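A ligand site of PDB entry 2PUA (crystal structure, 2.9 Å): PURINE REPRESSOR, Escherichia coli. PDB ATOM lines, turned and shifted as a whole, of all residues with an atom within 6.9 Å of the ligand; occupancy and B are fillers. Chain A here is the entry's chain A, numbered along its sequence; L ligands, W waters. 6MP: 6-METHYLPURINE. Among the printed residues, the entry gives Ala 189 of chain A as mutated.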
ATOM      1  N   THR A  66     -10.300   7.220  -3.050  1.00  0.00           N
ATOM      2  CA  THR A  66     -10.136   8.484  -2.346  1.00  0.00           C
ATOM      3  C   THR A  66     -11.133   8.588  -1.169  1.00  0.00           C
ATOM      4  O   THR A  66     -10.766   8.891  -0.052  1.00  0.00           O
ATOM      5  CB  THR A  66     -10.293   9.660  -3.288  1.00  0.00           C
ATOM      6  OG1 THR A  66      -9.102   9.799  -4.107  1.00  0.00           O
ATOM      7  CG2 THR A  66     -10.500  10.885  -2.478  1.00  0.00           C
ATOM      8  N   ALA A  70     -19.105   9.650  -1.630  1.00  0.00           N
ATOM      9  CA  ALA A  70     -19.380  10.497  -2.767  1.00  0.00           C
ATOM     10  C   ALA A  70     -20.074   9.786  -3.991  1.00  0.00           C
ATOM     11  O   ALA A  70     -19.639   8.736  -4.521  1.00  0.00           O
ATOM     12  CB  ALA A  70     -18.123  11.156  -3.164  1.00  0.00           C
ATOM     13  N   ALA A  71     -21.182  10.381  -4.387  1.00  0.00           N
ATOM     14  CA  ALA A  71     -22.023   9.887  -5.454  1.00  0.00           C
ATOM     15  C   ALA A  71     -21.239   9.302  -6.609  1.00  0.00           C
ATOM     16  O   ALA A  71     -21.446   8.158  -6.959  1.00  0.00           O
ATOM     17  CB  ALA A  71     -22.966  11.009  -5.964  1.00  0.00           C
ATOM     18  N   TYR A  72     -20.331  10.128  -7.140  1.00  0.00           N
ATOM     19  CA  TYR A  72     -19.473   9.837  -8.267  1.00  0.00           C
ATOM     20  C   TYR A  72     -18.800   8.508  -7.961  1.00  0.00           C
ATOM     21  O   TYR A  72     -19.109   7.401  -8.475  1.00  0.00           O
ATOM     22  CB  TYR A  72     -18.438  10.964  -8.281  1.00  0.00           C
ATOM     23  CG  TYR A  72     -17.514  10.877  -9.403  1.00  0.00           C
ATOM     24  CD1 TYR A  72     -17.974  11.044 -10.683  1.00  0.00           C
ATOM     25  CD2 TYR A  72     -16.175  10.603  -9.223  1.00  0.00           C
ATOM     26  CE1 TYR A  72     -17.137  10.955 -11.778  1.00  0.00           C
ATOM     27  CE2 TYR A  72     -15.310  10.512 -10.316  1.00  0.00           C
ATOM     28  CZ  TYR A  72     -15.819  10.690 -11.600  1.00  0.00           C
ATOM     29  OH  TYR A  72     -15.060  10.584 -12.714  1.00  0.00           O
ATOM     30  N   PHE A  73     -17.904   8.645  -7.039  1.00  0.00           N
ATOM     31  CA  PHE A  73     -17.142   7.551  -6.551  1.00  0.00           C
ATOM     32  C   PHE A  73     -17.877   6.255  -6.280  1.00  0.00           C
ATOM     33  O   PHE A  73     -17.485   5.177  -6.714  1.00  0.00           O
ATOM     34  CB  PHE A  73     -16.566   8.066  -5.273  1.00  0.00           C
ATOM     35  CG  PHE A  73     -15.398   8.951  -5.512  1.00  0.00           C
ATOM     36  CD1 PHE A  73     -14.576   8.691  -6.605  1.00  0.00           C
ATOM     37  CD2 PHE A  73     -15.094  10.035  -4.658  1.00  0.00           C
ATOM     38  CE1 PHE A  73     -13.482   9.462  -6.835  1.00  0.00           C
ATOM     39  CE2 PHE A  73     -13.985  10.818  -4.889  1.00  0.00           C
ATOM     40  CZ  PHE A  73     -13.185  10.520  -6.006  1.00  0.00           C
ATOM     41  N   ASN A  98      -6.944  11.106   0.599  1.00  0.00           N
ATOM     42  CA  ASN A  98      -5.910  12.046   0.162  1.00  0.00           C
ATOM     43  C   ASN A  98      -4.841  12.252   1.271  1.00  0.00           C
ATOM     44  O   ASN A  98      -4.160  13.265   1.317  1.00  0.00           O
ATOM     45  CB  ASN A  98      -6.517  13.374  -0.345  1.00  0.00           C
ATOM     46  CG  ASN A  98      -6.766  13.378  -1.851  1.00  0.00           C
ATOM     47  OD1 ASN A  98      -7.907  13.483  -2.298  1.00  0.00           O
ATOM     48  ND2 ASN A  98      -5.685  13.244  -2.643  1.00  0.00           N
ATOM     49  N   CYS A 122      -6.835   8.164  -6.691  1.00  0.00           N
ATOM     50  CA  CYS A 122      -6.485   9.081  -5.620  1.00  0.00           C
ATOM     51  C   CYS A 122      -6.763  10.531  -5.813  1.00  0.00           C
ATOM     52  O   CYS A 122      -6.355  11.385  -5.013  1.00  0.00           O
ATOM     53  CB  CYS A 122      -5.052   8.828  -5.166  1.00  0.00           C
ATOM     54  SG  CYS A 122      -4.940   7.172  -4.420  1.00  0.00           S
ATOM     55  N   SER A 123      -7.479  10.835  -6.874  1.00  0.00           N
ATOM     56  CA  SER A 123      -7.838  12.216  -7.127  1.00  0.00           C
ATOM     57  C   SER A 123      -6.609  13.073  -7.369  1.00  0.00           C
ATOM     58  O   SER A 123      -6.272  13.335  -8.506  1.00  0.00           O
ATOM     59  CB  SER A 123      -8.689  12.753  -5.996  1.00  0.00           C
ATOM     60  OG  SER A 123      -9.886  12.025  -5.900  1.00  0.00           O
ATOM     61  N   GLU A 124      -5.913  13.517  -6.339  1.00  0.00           N
ATOM     62  CA  GLU A 124      -4.737  14.326  -6.593  1.00  0.00           C
ATOM     63  C   GLU A 124      -3.521  13.416  -6.592  1.00  0.00           C
ATOM     64  O   GLU A 124      -3.545  12.372  -5.926  1.00  0.00           O
ATOM     65  CB  GLU A 124      -4.616  15.437  -5.567  1.00  0.00           C
ATOM     66  CG  GLU A 124      -5.988  15.934  -5.149  1.00  0.00           C
ATOM     67  CD  GLU A 124      -5.875  17.071  -4.220  1.00  0.00           C
ATOM     68  OE1 GLU A 124      -4.770  17.262  -3.678  1.00  0.00           O
ATOM     69  OE2 GLU A 124      -6.864  17.809  -4.058  1.00  0.00           O
ATOM     70  N   ASP A 145      -8.005   7.497 -12.971  1.00  0.00           N
ATOM     71  CA  ASP A 145      -8.261   8.934 -13.069  1.00  0.00           C
ATOM     72  C   ASP A 145      -7.181   9.949 -13.467  1.00  0.00           C
ATOM     73  O   ASP A 145      -7.100  11.016 -12.852  1.00  0.00           O
ATOM     74  CB  ASP A 145      -8.913   9.411 -11.767  1.00  0.00           C
ATOM     75  CG  ASP A 145      -8.009   9.174 -10.519  1.00  0.00           C
ATOM     76  OD1 ASP A 145      -6.812   8.841 -10.729  1.00  0.00           O
ATOM     77  OD2 ASP A 145      -8.510   9.339  -9.346  1.00  0.00           O
ATOM     78  N   PRO A 186     -11.455  21.341  -7.180  1.00  0.00           N
ATOM     79  CA  PRO A 186     -10.005  21.550  -6.985  1.00  0.00           C
ATOM     80  C   PRO A 186      -9.086  21.350  -8.178  1.00  0.00           C
ATOM     81  O   PRO A 186      -9.135  20.298  -8.846  1.00  0.00           O
ATOM     82  CB  PRO A 186      -9.629  20.524  -5.902  1.00  0.00           C
ATOM     83  CG  PRO A 186     -10.743  19.538  -5.907  1.00  0.00           C
ATOM     84  CD  PRO A 186     -11.987  20.320  -6.262  1.00  0.00           C
ATOM     85  N   ALA A 189      -6.828  18.178  -9.005  1.00  0.00           N
ATOM     86  CA  ALA A 189      -7.302  16.926  -9.610  1.00  0.00           C
ATOM     87  C   ALA A 189      -7.704  17.172 -11.055  1.00  0.00           C
ATOM     88  O   ALA A 189      -7.946  18.320 -11.495  1.00  0.00           O
ATOM     89  CB  ALA A 189      -8.438  16.321  -8.822  1.00  0.00           C
ATOM     90  N   ASN A 190      -7.752  16.078 -11.797  1.00  0.00           N
ATOM     91  CA  ASN A 190      -8.075  16.108 -13.199  1.00  0.00           C
ATOM     92  C   ASN A 190      -9.466  16.636 -13.480  1.00  0.00           C
ATOM     93  O   ASN A 190      -9.655  17.647 -14.198  1.00  0.00           O
ATOM     94  CB  ASN A 190      -7.914  14.678 -13.737  1.00  0.00           C
ATOM     95  CG  ASN A 190      -8.334  14.552 -15.174  1.00  0.00           C
ATOM     96  OD1 ASN A 190      -7.949  15.382 -16.031  1.00  0.00           O
ATOM     97  ND2 ASN A 190      -9.188  13.520 -15.487  1.00  0.00           N
ATOM     98  N   THR A 191     -10.430  15.935 -12.882  1.00  0.00           N
ATOM     99  CA  THR A 191     -11.841  16.244 -12.990  1.00  0.00           C
ATOM    100  C   THR A 191     -12.063  17.658 -12.533  1.00  0.00           C
ATOM    101  O   THR A 191     -13.174  18.192 -12.714  1.00  0.00           O
ATOM    102  CB  THR A 191     -12.630  15.359 -12.097  1.00  0.00           C
ATOM    103  OG1 THR A 191     -12.073  15.427 -10.787  1.00  0.00           O
ATOM    104  CG2 THR A 191     -12.585  13.918 -12.596  1.00  0.00           C
ATOM    105  N   GLY A 192     -11.034  18.269 -11.910  1.00  0.00           N
ATOM    106  CA  GLY A 192     -11.091  19.623 -11.455  1.00  0.00           C
ATOM    107  C   GLY A 192     -10.507  20.435 -12.617  1.00  0.00           C
ATOM    108  O   GLY A 192     -11.182  20.764 -13.599  1.00  0.00           O
ATOM    109  N   ARG A 195     -11.594  19.844 -16.383  1.00  0.00           N
ATOM    110  CA  ARG A 195     -12.901  20.225 -16.867  1.00  0.00           C
ATOM    111  C   ARG A 195     -12.883  21.744 -17.042  1.00  0.00           C
ATOM    112  O   ARG A 195     -13.400  22.243 -18.041  1.00  0.00           O
ATOM    113  CB  ARG A 195     -13.993  19.752 -15.889  1.00  0.00           C
ATOM    114  CG  ARG A 195     -14.075  18.234 -15.707  1.00  0.00           C
ATOM    115  CD  ARG A 195     -15.140  17.759 -14.727  1.00  0.00           C
ATOM    116  NE  ARG A 195     -15.232  16.298 -14.668  1.00  0.00           N
ATOM    117  CZ  ARG A 195     -16.076  15.620 -13.887  1.00  0.00           C
ATOM    118  NH1 ARG A 195     -16.909  16.263 -13.070  1.00  0.00           N
ATOM    119  NH2 ARG A 195     -16.062  14.289 -13.889  1.00  0.00           N
ATOM    120  N   ASP A 219     -15.238  21.876  -3.748  1.00  0.00           N
ATOM    121  CA  ASP A 219     -14.426  20.746  -3.312  1.00  0.00           C
ATOM    122  C   ASP A 219     -15.148  19.484  -3.669  1.00  0.00           C
ATOM    123  O   ASP A 219     -14.840  18.430  -3.122  1.00  0.00           O
ATOM    124  CB  ASP A 219     -14.205  20.826  -1.802  1.00  0.00           C
ATOM    125  CG  ASP A 219     -15.503  20.827  -1.023  1.00  0.00           C
ATOM    126  OD1 ASP A 219     -16.606  20.628  -1.605  1.00  0.00           O
ATOM    127  OD2 ASP A 219     -15.436  21.079   0.174  1.00  0.00           O
ATOM    128  N   PHE A 220     -16.122  19.604  -4.571  1.00  0.00           N
ATOM    129  CA  PHE A 220     -16.982  18.496  -5.023  1.00  0.00           C
ATOM    130  C   PHE A 220     -18.065  18.242  -3.994  1.00  0.00           C
ATOM    131  O   PHE A 220     -18.917  17.403  -4.161  1.00  0.00           O
ATOM    132  CB  PHE A 220     -16.201  17.235  -5.307  1.00  0.00           C
ATOM    133  CG  PHE A 220     -15.385  17.330  -6.518  1.00  0.00           C
ATOM    134  CD1 PHE A 220     -15.969  17.578  -7.736  1.00  0.00           C
ATOM    135  CD2 PHE A 220     -14.019  17.231  -6.431  1.00  0.00           C
ATOM    136  CE1 PHE A 220     -15.197  17.691  -8.871  1.00  0.00           C
ATOM    137  CE2 PHE A 220     -13.234  17.344  -7.555  1.00  0.00           C
ATOM    138  CZ  PHE A 220     -13.827  17.570  -8.780  1.00  0.00           C
ATOM    139  N   GLU A 221     -18.034  19.008  -2.927  1.00  0.00           N
ATOM    140  CA  GLU A 221     -19.022  18.874  -1.897  1.00  0.00           C
ATOM    141  C   GLU A 221     -20.096  20.004  -1.925  1.00  0.00           C
ATOM    142  O   GLU A 221     -19.863  21.236  -2.058  1.00  0.00           O
ATOM    143  CB  GLU A 221     -18.342  18.737  -0.544  1.00  0.00           C
ATOM    144  CG  GLU A 221     -17.505  17.485  -0.399  1.00  0.00           C
ATOM    145  CD  GLU A 221     -18.062  16.497   0.644  1.00  0.00           C
ATOM    146  OE1 GLU A 221     -19.215  16.040   0.476  1.00  0.00           O
ATOM    147  OE2 GLU A 221     -17.363  16.204   1.640  1.00  0.00           O
ATOM    148  N   GLY A 245     -18.563  22.385 -11.915  1.00  0.00           N
ATOM    149  CA  GLY A 245     -17.564  21.282 -11.895  1.00  0.00           C
ATOM    150  C   GLY A 245     -17.990  19.843 -11.658  1.00  0.00           C
ATOM    151  O   GLY A 245     -17.353  18.927 -12.175  1.00  0.00           O
ATOM    152  N   GLY A 246     -19.051  19.638 -10.852  1.00  0.00           N
ATOM    153  CA  GLY A 246     -19.642  18.313 -10.550  1.00  0.00           C
ATOM    154  C   GLY A 246     -21.152  18.445 -10.109  1.00  0.00           C
ATOM    155  O   GLY A 246     -21.557  19.466  -9.522  1.00  0.00           O
ATOM    156  N   ASP A 247     -21.990  17.445 -10.397  1.00  0.00           N
ATOM    157  CA  ASP A 247     -23.407  17.489  -9.987  1.00  0.00           C
ATOM    158  C   ASP A 247     -23.705  17.685  -8.426  1.00  0.00           C
ATOM    159  O   ASP A 247     -24.679  18.363  -7.998  1.00  0.00           O
ATOM    160  CB  ASP A 247     -24.106  16.166 -10.352  1.00  0.00           C
ATOM    161  CG  ASP A 247     -24.137  15.867 -11.895  1.00  0.00           C
ATOM    162  OD1 ASP A 247     -23.415  16.596 -12.578  1.00  0.00           O
ATOM    163  OD2 ASP A 247     -24.707  14.869 -12.429  1.00  0.00           O
ATOM    164  N   ILE A 248     -22.939  17.021  -7.570  1.00  0.00           N
ATOM    165  CA  ILE A 248     -23.255  17.168  -6.163  1.00  0.00           C
ATOM    166  C   ILE A 248     -23.058  18.598  -5.673  1.00  0.00           C
ATOM    167  O   ILE A 248     -23.756  19.101  -4.805  1.00  0.00           O
ATOM    168  CB  ILE A 248     -22.519  16.165  -5.275  1.00  0.00           C
ATOM    169  CG1 ILE A 248     -22.813  14.721  -5.694  1.00  0.00           C
ATOM    170  CG2 ILE A 248     -22.912  16.428  -3.831  1.00  0.00           C
ATOM    171  CD1 ILE A 248     -24.193  14.274  -5.424  1.00  0.00           C
ATOM    172  N   TYR A 273     -21.912  18.527 -14.133  1.00  0.00           N
ATOM    173  CA  TYR A 273     -20.965  17.600 -14.749  1.00  0.00           C
ATOM    174  C   TYR A 273     -20.837  16.344 -13.937  1.00  0.00           C
ATOM    175  O   TYR A 273     -20.560  16.467 -12.749  1.00  0.00           O
ATOM    176  CB  TYR A 273     -19.602  18.196 -14.692  1.00  0.00           C
ATOM    177  CG  TYR A 273     -18.692  17.604 -15.699  1.00  0.00           C
ATOM    178  CD1 TYR A 273     -18.613  16.226 -15.924  1.00  0.00           C
ATOM    179  CD2 TYR A 273     -17.863  18.444 -16.470  1.00  0.00           C
ATOM    180  CE1 TYR A 273     -17.728  15.705 -16.874  1.00  0.00           C
ATOM    181  CE2 TYR A 273     -16.989  17.954 -17.416  1.00  0.00           C
ATOM    182  CZ  TYR A 273     -16.924  16.594 -17.625  1.00  0.00           C
ATOM    183  OH  TYR A 273     -16.052  16.169 -18.573  1.00  0.00           O
ATOM    184  N   ASP A 274     -20.994  15.189 -14.599  1.00  0.00           N
ATOM    185  CA  ASP A 274     -20.856  13.805 -14.047  1.00  0.00           C
ATOM    186  C   ASP A 274     -22.030  12.921 -14.389  1.00  0.00           C
ATOM    187  O   ASP A 274     -21.946  11.712 -14.707  1.00  0.00           O
ATOM    188  CB  ASP A 274     -20.745  13.766 -12.529  1.00  0.00           C
ATOM    189  CG  ASP A 274     -19.338  14.092 -12.001  1.00  0.00           C
ATOM    190  OD1 ASP A 274     -18.339  14.090 -12.780  1.00  0.00           O
ATOM    191  OD2 ASP A 274     -19.259  14.335 -10.771  1.00  0.00           O
ATOM    192  N   GLN A 291     -20.470  11.523 -17.339  1.00  0.00           N
ATOM    193  CA  GLN A 291     -19.257  10.782 -17.288  1.00  0.00           C
ATOM    194  C   GLN A 291     -19.707   9.337 -17.285  1.00  0.00           C
ATOM    195  O   GLN A 291     -20.516   8.942 -16.444  1.00  0.00           O
ATOM    196  CB  GLN A 291     -18.570  10.965 -15.954  1.00  0.00           C
ATOM    197  CG  GLN A 291     -17.341  10.062 -15.791  1.00  0.00           C
ATOM    198  CD  GLN A 291     -16.109  10.697 -16.449  1.00  0.00           C
ATOM    199  OE1 GLN A 291     -15.238  11.239 -15.767  1.00  0.00           O
ATOM    200  NE2 GLN A 291     -16.102  10.729 -17.788  1.00  0.00           N
HETATM  201  N9  6MP L   1     -16.584  14.064  -9.618  1.00  0.00           N
HETATM  202  C4  6MP L   1     -16.155  13.968  -8.322  1.00  0.00           C
HETATM  203  N3  6MP L   1     -16.937  13.863  -7.230  1.00  0.00           N
HETATM  204  C2  6MP L   1     -16.225  13.808  -6.115  1.00  0.00           C
HETATM  205  N1  6MP L   1     -14.846  13.828  -6.080  1.00  0.00           N
HETATM  206  C6  6MP L   1     -14.029  13.904  -7.196  1.00  0.00           C
HETATM  207  C7  6MP L   1     -12.497  13.882  -7.036  1.00  0.00           C
HETATM  208  C5  6MP L   1     -14.778  13.991  -8.390  1.00  0.00           C
HETATM  209  N7  6MP L   1     -14.345  14.111  -9.701  1.00  0.00           N
HETATM  210  C8  6MP L   1     -15.450  14.153 -10.389  1.00  0.00           C
HETATM  211  O   HOH W   1     -13.937  14.554  -3.069  1.00  0.00           O
HETATM  212  O   HOH W   2     -19.918  12.496  -6.118  1.00  0.00           O
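A nitrogen (N9) of the ligand sits close to the side-chain carboxylate (OD2) of Asp 274 (2.9 Å). OG1 of Thr 191 is in hydrogen-bond range of N7 of the ligand, at 2.8 Å.
O of Asp 274 is in hydrogen-bond range of N of Gln 291 (3.0 Å). The guanidinium group (NH2) of Arg 195 lies within salt-bridge range of the side-chain carboxylate (OD1) of Asp 274, 2.5 Å away. N of Asp 274 is in hydrogen-bond range of OD1 of Asp 247. N of Ser 123 lies within hydrogen-bond range of OD2 of Asp 145 (3.1 Å). The guanidinium group (NH1) of Arg 195 lies within hydrogen-bond range of the backbone carbonyl oxygen (O) of Gly 245 (2.8 Å). OH of Tyr 72 lies within hydrogen-bond range of OE1 of Gln 291, 3.1 Å away. OG1 of Thr 66 is in hydrogen-bond range of OG of Ser 123 (3.0 Å). The backbone carbonyl oxygen of Thr 191 sits close to the guanidinium group of Arg 195, 3.4 Å away.
Residues that only touch the ligand: Tyr 72, Phe 73, Ser 123, Arg 195 and Phe 220. Of the 26 residues printed, 7 come within 4 Å of the ligand. The nearest printed residue that does not touch the ligand is Ala 70 (4.4 Å).
Water W2 lies within hydrogen-bond range of the backbone NH of Tyr 72 (2.6 Å), the backbone NH of Ala 71 (3.0 Å) and a nitrogen (N3) of the ligand (3.5 Å).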
